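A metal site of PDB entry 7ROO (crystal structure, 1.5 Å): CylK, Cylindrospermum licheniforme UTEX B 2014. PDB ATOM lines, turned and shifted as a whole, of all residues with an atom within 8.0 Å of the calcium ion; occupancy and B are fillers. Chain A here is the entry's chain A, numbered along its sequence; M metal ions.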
ATOM      1  N   ASP A 115      22.159 -25.855 -23.374  1.00  0.00           N
ATOM      2  CA  ASP A 115      21.568 -26.398 -22.127  1.00  0.00           C
ATOM      3  C   ASP A 115      22.613 -26.229 -21.024  1.00  0.00           C
ATOM      4  O   ASP A 115      23.607 -26.965 -20.989  1.00  0.00           O
ATOM      5  CB  ASP A 115      21.102 -27.832 -22.250  1.00  0.00           C
ATOM      6  CG  ASP A 115      20.228 -28.192 -21.061  1.00  0.00           C
ATOM      7  OD1 ASP A 115      20.639 -27.784 -19.965  1.00  0.00           O
ATOM      8  OD2 ASP A 115      19.146 -28.805 -21.265  1.00  0.00           O
ATOM      9  N   PRO A 116      22.399 -25.289 -20.094  1.00  0.00           N
ATOM     10  CA  PRO A 116      23.398 -24.975 -19.071  1.00  0.00           C
ATOM     11  C   PRO A 116      23.500 -26.071 -18.008  1.00  0.00           C
ATOM     12  O   PRO A 116      24.422 -26.055 -17.214  1.00  0.00           O
ATOM     13  CB  PRO A 116      22.904 -23.651 -18.439  1.00  0.00           C
ATOM     14  CG  PRO A 116      21.427 -23.698 -18.648  1.00  0.00           C
ATOM     15  CD  PRO A 116      21.202 -24.423 -19.949  1.00  0.00           C
ATOM     16  N   GLY A 117      22.578 -27.034 -18.050  1.00  0.00           N
ATOM     17  CA  GLY A 117      22.634 -28.149 -17.101  1.00  0.00           C
ATOM     18  C   GLY A 117      23.234 -29.395 -17.706  1.00  0.00           C
ATOM     19  O   GLY A 117      23.439 -30.357 -16.955  1.00  0.00           O
ATOM     20  N   ASP A 159      21.448 -16.832 -18.618  1.00  0.00           N
ATOM     21  CA  ASP A 159      20.275 -16.663 -17.730  1.00  0.00           C
ATOM     22  C   ASP A 159      20.783 -16.138 -16.395  1.00  0.00           C
ATOM     23  O   ASP A 159      21.955 -15.762 -16.325  1.00  0.00           O
ATOM     24  CB  ASP A 159      19.464 -17.952 -17.650  1.00  0.00           C
ATOM     25  CG  ASP A 159      20.267 -19.175 -17.219  1.00  0.00           C
ATOM     26  OD1 ASP A 159      21.205 -18.976 -16.387  1.00  0.00           O
ATOM     27  OD2 ASP A 159      20.067 -20.285 -17.802  1.00  0.00           O
ATOM     28  N   GLN A 161      21.602 -17.726 -13.895  1.00  0.00           N
ATOM     29  CA  GLN A 161      22.523 -18.654 -13.234  1.00  0.00           C
ATOM     30  C   GLN A 161      23.932 -18.523 -13.809  1.00  0.00           C
ATOM     31  O   GLN A 161      24.901 -18.584 -13.025  1.00  0.00           O
ATOM     32  CB  GLN A 161      21.978 -20.076 -13.370  1.00  0.00           C
ATOM     33  CG  GLN A 161      22.824 -21.139 -12.699  1.00  0.00           C
ATOM     34  CD  GLN A 161      21.949 -22.131 -11.977  1.00  0.00           C
ATOM     35  OE1 GLN A 161      21.118 -22.822 -12.580  1.00  0.00           O
ATOM     36  NE2 GLN A 161      22.160 -22.229 -10.678  1.00  0.00           N
ATOM     37  N   HIS A 254       5.857 -27.567  -9.245  1.00  0.00           N
ATOM     38  CA  HIS A 254       7.097 -27.107  -9.898  1.00  0.00           C
ATOM     39  C   HIS A 254       7.912 -28.356 -10.291  1.00  0.00           C
ATOM     40  O   HIS A 254       8.218 -29.174  -9.439  1.00  0.00           O
ATOM     41  CB  HIS A 254       7.908 -26.192  -8.993  1.00  0.00           C
ATOM     42  CG  HIS A 254       9.225 -25.844  -9.616  1.00  0.00           C
ATOM     43  ND1 HIS A 254      10.349 -26.647  -9.440  1.00  0.00           N
ATOM     44  CD2 HIS A 254       9.610 -24.760 -10.356  1.00  0.00           C
ATOM     45  CE1 HIS A 254      11.366 -26.081 -10.110  1.00  0.00           C
ATOM     46  NE2 HIS A 254      10.918 -24.966 -10.702  1.00  0.00           N
ATOM     47  N   ILE A 255       8.376 -28.401 -11.531  1.00  0.00           N
ATOM     48  CA  ILE A 255       9.177 -29.526 -12.068  1.00  0.00           C
ATOM     49  C   ILE A 255      10.403 -28.892 -12.702  1.00  0.00           C
ATOM     50  O   ILE A 255      10.248 -28.159 -13.702  1.00  0.00           O
ATOM     51  CB  ILE A 255       8.348 -30.388 -13.017  1.00  0.00           C
ATOM     52  CG1 ILE A 255       7.246 -31.107 -12.229  1.00  0.00           C
ATOM     53  CG2 ILE A 255       9.287 -31.370 -13.737  1.00  0.00           C
ATOM     54  CD1 ILE A 255       6.271 -31.880 -13.067  1.00  0.00           C
ATOM     55  N   GLY A 256      11.591 -29.160 -12.192  1.00  0.00           N
ATOM     56  CA  GLY A 256      12.784 -28.592 -12.822  1.00  0.00           C
ATOM     57  C   GLY A 256      14.072 -29.176 -12.298  1.00  0.00           C
ATOM     58  O   GLY A 256      14.206 -29.496 -11.108  1.00  0.00           O
ATOM     59  N   THR A 257      15.023 -29.219 -13.225  1.00  0.00           N
ATOM     60  CA  THR A 257      16.464 -29.461 -13.004  1.00  0.00           C
ATOM     61  C   THR A 257      17.238 -28.245 -13.505  1.00  0.00           C
ATOM     62  O   THR A 257      16.659 -27.268 -14.021  1.00  0.00           O
ATOM     63  CB  THR A 257      16.952 -30.709 -13.800  1.00  0.00           C
ATOM     64  OG1 THR A 257      17.031 -30.421 -15.203  1.00  0.00           O
ATOM     65  CG2 THR A 257      16.083 -31.912 -13.543  1.00  0.00           C
ATOM     66  N   ALA A 258      18.568 -28.261 -13.357  1.00  0.00           N
ATOM     67  CA  ALA A 258      19.430 -27.198 -13.860  1.00  0.00           C
ATOM     68  C   ALA A 258      19.406 -27.172 -15.396  1.00  0.00           C
ATOM     69  O   ALA A 258      19.904 -26.173 -15.928  1.00  0.00           O
ATOM     70  CB  ALA A 258      20.844 -27.437 -13.383  1.00  0.00           C
ATOM     71  N   ALA A 259      18.866 -28.231 -16.038  1.00  0.00           N
ATOM     72  CA  ALA A 259      18.828 -28.314 -17.515  1.00  0.00           C
ATOM     73  C   ALA A 259      17.523 -27.705 -18.063  1.00  0.00           C
ATOM     74  O   ALA A 259      16.704 -27.110 -17.333  1.00  0.00           O
ATOM     75  CB  ALA A 259      19.007 -29.761 -18.001  1.00  0.00           C
ATOM     76  N   ASN A 260      17.322 -27.806 -19.346  1.00  0.00           N
ATOM     77  CA  ASN A 260      16.047 -27.356 -19.967  1.00  0.00           C
ATOM     78  C   ASN A 260      14.976 -28.442 -19.796  1.00  0.00           C
ATOM     79  O   ASN A 260      15.128 -29.553 -20.382  1.00  0.00           O
ATOM     80  CB  ASN A 260      16.298 -27.007 -21.440  1.00  0.00           C
ATOM     81  CG  ASN A 260      17.215 -25.826 -21.633  1.00  0.00           C
ATOM     82  OD1 ASN A 260      17.063 -24.856 -20.873  1.00  0.00           O
ATOM     83  ND2 ASN A 260      18.019 -25.798 -22.702  1.00  0.00           N
ATOM     84  N   ASP A 261      13.884 -28.181 -19.063  1.00  0.00           N
ATOM     85  CA  ASP A 261      12.837 -29.165 -18.714  1.00  0.00           C
ATOM     86  C   ASP A 261      11.488 -28.704 -19.236  1.00  0.00           C
ATOM     87  O   ASP A 261      11.117 -27.524 -18.959  1.00  0.00           O
ATOM     88  CB  ASP A 261      12.738 -29.367 -17.214  1.00  0.00           C
ATOM     89  CG  ASP A 261      14.080 -29.454 -16.502  1.00  0.00           C
ATOM     90  OD1 ASP A 261      14.752 -30.514 -16.699  1.00  0.00           O
ATOM     91  OD2 ASP A 261      14.479 -28.455 -15.854  1.00  0.00           O
ATOM     92  N   TYR A 262      10.777 -29.576 -19.918  1.00  0.00           N
ATOM     93  CA  TYR A 262       9.520 -29.231 -20.614  1.00  0.00           C
ATOM     94  C   TYR A 262       8.425 -30.235 -20.309  1.00  0.00           C
ATOM     95  O   TYR A 262       8.643 -31.427 -20.466  1.00  0.00           O
ATOM     96  CB  TYR A 262       9.726 -29.159 -22.126  1.00  0.00           C
ATOM     97  CG  TYR A 262      10.850 -28.245 -22.568  1.00  0.00           C
ATOM     98  CD1 TYR A 262      12.140 -28.723 -22.693  1.00  0.00           C
ATOM     99  CD2 TYR A 262      10.662 -26.884 -22.795  1.00  0.00           C
ATOM    100  CE1 TYR A 262      13.188 -27.887 -23.052  1.00  0.00           C
ATOM    101  CE2 TYR A 262      11.694 -26.036 -23.144  1.00  0.00           C
ATOM    102  CZ  TYR A 262      12.964 -26.546 -23.271  1.00  0.00           C
ATOM    103  OH  TYR A 262      14.019 -25.706 -23.564  1.00  0.00           O
ATOM    104  N   THR A 280      13.456 -33.454 -21.398  1.00  0.00           N
ATOM    105  CA  THR A 280      14.407 -32.818 -20.429  1.00  0.00           C
ATOM    106  C   THR A 280      15.843 -33.014 -20.892  1.00  0.00           C
ATOM    107  O   THR A 280      16.171 -34.165 -21.316  1.00  0.00           O
ATOM    108  CB  THR A 280      14.185 -33.338 -18.996  1.00  0.00           C
ATOM    109  OG1 THR A 280      15.113 -32.731 -18.109  1.00  0.00           O
ATOM    110  CG2 THR A 280      14.367 -34.835 -18.959  1.00  0.00           C
ATOM    111  N   GLY A 281      16.679 -31.988 -20.683  1.00  0.00           N
ATOM    112  CA  GLY A 281      18.139 -32.125 -20.845  1.00  0.00           C
ATOM    113  C   GLY A 281      18.828 -32.534 -19.582  1.00  0.00           C
ATOM    114  O   GLY A 281      20.053 -32.646 -19.611  1.00  0.00           O
ATOM    115  N   GLY A 282      18.062 -32.837 -18.541  1.00  0.00           N
ATOM    116  CA  GLY A 282      18.629 -33.169 -17.239  1.00  0.00           C
ATOM    117  C   GLY A 282      18.318 -34.594 -16.794  1.00  0.00           C
ATOM    118  O   GLY A 282      17.809 -35.392 -17.574  1.00  0.00           O
ATOM    119  N   LEU A 284      15.771 -35.874 -14.637  1.00  0.00           N
ATOM    120  CA  LEU A 284      14.473 -35.469 -14.042  1.00  0.00           C
ATOM    121  C   LEU A 284      13.739 -36.708 -13.519  1.00  0.00           C
ATOM    122  O   LEU A 284      13.504 -36.779 -12.289  1.00  0.00           O
ATOM    123  CB  LEU A 284      13.661 -34.723 -15.132  1.00  0.00           C
ATOM    124  CG  LEU A 284      12.327 -34.086 -14.685  1.00  0.00           C
ATOM    125  CD1 LEU A 284      11.749 -33.265 -15.833  1.00  0.00           C
ATOM    126  CD2 LEU A 284      11.303 -35.123 -14.285  1.00  0.00           C
ATOM    127  N   THR A 631       8.334 -22.375 -18.345  1.00  0.00           N
ATOM    128  CA  THR A 631       8.682 -21.013 -17.909  1.00  0.00           C
ATOM    129  C   THR A 631      10.199 -20.801 -17.815  1.00  0.00           C
ATOM    130  O   THR A 631      10.958 -21.791 -17.549  1.00  0.00           O
ATOM    131  CB  THR A 631       8.061 -20.764 -16.532  1.00  0.00           C
ATOM    132  OG1 THR A 631       8.270 -19.377 -16.234  1.00  0.00           O
ATOM    133  CG2 THR A 631       8.649 -21.583 -15.413  1.00  0.00           C
ATOM    134  N   ASN A 639      13.235 -21.058  -9.772  1.00  0.00           N
ATOM    135  CA  ASN A 639      13.797 -21.662 -11.013  1.00  0.00           C
ATOM    136  C   ASN A 639      15.090 -22.433 -10.722  1.00  0.00           C
ATOM    137  O   ASN A 639      15.976 -21.896 -10.034  1.00  0.00           O
ATOM    138  CB  ASN A 639      14.010 -20.554 -12.033  1.00  0.00           C
ATOM    139  CG  ASN A 639      14.433 -21.109 -13.377  1.00  0.00           C
ATOM    140  OD1 ASN A 639      15.618 -21.383 -13.566  1.00  0.00           O
ATOM    141  ND2 ASN A 639      13.486 -21.195 -14.310  1.00  0.00           N
ATOM    142  N   ALA A 640      15.178 -23.679 -11.178  1.00  0.00           N
ATOM    143  CA  ALA A 640      16.304 -24.613 -10.989  1.00  0.00           C
ATOM    144  C   ALA A 640      17.370 -24.395 -12.066  1.00  0.00           C
ATOM    145  O   ALA A 640      18.543 -24.835 -11.858  1.00  0.00           O
ATOM    146  CB  ALA A 640      15.831 -26.018 -11.037  1.00  0.00           C
ATOM    147  N   GLY A 641      17.025 -23.723 -13.159  1.00  0.00           N
ATOM    148  CA  GLY A 641      17.941 -23.359 -14.234  1.00  0.00           C
ATOM    149  C   GLY A 641      17.206 -23.344 -15.566  1.00  0.00           C
ATOM    150  O   GLY A 641      16.440 -24.266 -15.809  1.00  0.00           O
ATOM    151  N   SER A 642      17.442 -22.328 -16.354  1.00  0.00           N
ATOM    152  CA  SER A 642      16.874 -22.153 -17.711  1.00  0.00           C
ATOM    153  C   SER A 642      15.373 -22.491 -17.685  1.00  0.00           C
ATOM    154  O   SER A 642      14.597 -21.879 -16.875  1.00  0.00           O
ATOM    155  CB  SER A 642      17.683 -22.927 -18.643  1.00  0.00           C
ATOM    156  OG  SER A 642      17.332 -22.565 -19.995  1.00  0.00           O
ATOM    157  N   TYR A 643      14.884 -23.332 -18.582  1.00  0.00           N
ATOM    158  CA  TYR A 643      13.485 -23.701 -18.626  1.00  0.00           C
ATOM    159  C   TYR A 643      13.189 -24.685 -17.505  1.00  0.00           C
ATOM    160  O   TYR A 643      13.875 -25.730 -17.352  1.00  0.00           O
ATOM    161  CB  TYR A 643      13.093 -24.258 -20.006  1.00  0.00           C
ATOM    162  CG  TYR A 643      12.760 -23.164 -20.986  1.00  0.00           C
ATOM    163  CD1 TYR A 643      13.732 -22.472 -21.679  1.00  0.00           C
ATOM    164  CD2 TYR A 643      11.445 -22.830 -21.225  1.00  0.00           C
ATOM    165  CE1 TYR A 643      13.422 -21.474 -22.586  1.00  0.00           C
ATOM    166  CE2 TYR A 643      11.122 -21.780 -22.063  1.00  0.00           C
ATOM    167  CZ  TYR A 643      12.098 -21.104 -22.772  1.00  0.00           C
ATOM    168  OH  TYR A 643      11.754 -20.079 -23.634  1.00  0.00           O
ATOM    169  N   ASP A 644      12.099 -24.370 -16.826  1.00  0.00           N
ATOM    170  CA  ASP A 644      11.425 -25.264 -15.865  1.00  0.00           C
ATOM    171  C   ASP A 644       9.957 -25.475 -16.296  1.00  0.00           C
ATOM    172  O   ASP A 644       9.470 -24.731 -17.190  1.00  0.00           O
ATOM    173  CB  ASP A 644      11.496 -24.810 -14.404  1.00  0.00           C
ATOM    174  CG  ASP A 644      12.829 -24.902 -13.688  1.00  0.00           C
ATOM    175  OD1 ASP A 644      13.772 -25.457 -14.255  1.00  0.00           O
ATOM    176  OD2 ASP A 644      12.867 -24.447 -12.518  1.00  0.00           O
ATOM    177  N   SER A 645       9.281 -26.400 -15.658  1.00  0.00           N
ATOM    178  CA  SER A 645       7.876 -26.679 -16.004  1.00  0.00           C
ATOM    179  C   SER A 645       7.007 -26.554 -14.761  1.00  0.00           C
ATOM    180  O   SER A 645       7.525 -26.534 -13.603  1.00  0.00           O
ATOM    181  CB  SER A 645       7.784 -28.029 -16.687  1.00  0.00           C
ATOM    182  OG  SER A 645       8.411 -27.913 -17.961  1.00  0.00           O
HETATM  183 CA    CA M   1      15.363 -26.302 -15.664  1.00  0.00          CA
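The side-chain hydroxyl (OG1) of Thr 257 is in hydrogen-bond range of the backbone NH (N) of Ala 259, at 3.0 Å. The backbone NH of Ala 640 lies within hydrogen-bond range of the side-chain carboxylate of Asp 644, at 2.8 Å. The backbone carbonyl oxygen of Asp 644 lies within hydrogen-bond range of the backbone NH of Thr 631, 2.9 Å away. The side-chain carboxylate (OD1) of Asp 261 lies within hydrogen-bond range of the side-chain hydroxyl (OG1) of Thr 280, 2.7 Å away. The backbone NH (N) of Gly 641 sits at hydrogen-bond distance from the side-chain amide oxygen (OD1) of Asn 639 (2.8 Å). The backbone carbonyl oxygen (O) of Asp 261 lies within hydrogen-bond range of the side-chain hydroxyl (OG) of Ser 645. OD2 of Asp 644 lies within hydrogen-bond range of NE2 of His 254 (2.7 Å).
Within 4 Å of the calcium ion: Thr 257, Ala 259, Asp 261, Gly 641, Tyr 643 and Asp 644. The nearest printed residue that does not touch the calcium ion is Ala 258 (4.1 Å).
The calcium ion is bound by the side-chain carboxylate (OD1) of Asp 644 (2.3 Å), the backbone carbonyl oxygen (O) of Ala 259 (2.3 Å), the backbone carbonyl oxygen (O) of Thr 257 (2.3 Å), the backbone carbonyl oxygen (O) of Gly 641 (2.3 Å), the backbone carbonyl oxygen (O) of Tyr 643 (2.3 Å) and the side-chain carboxylate (OD2) of Asp 261 (2.3 Å).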
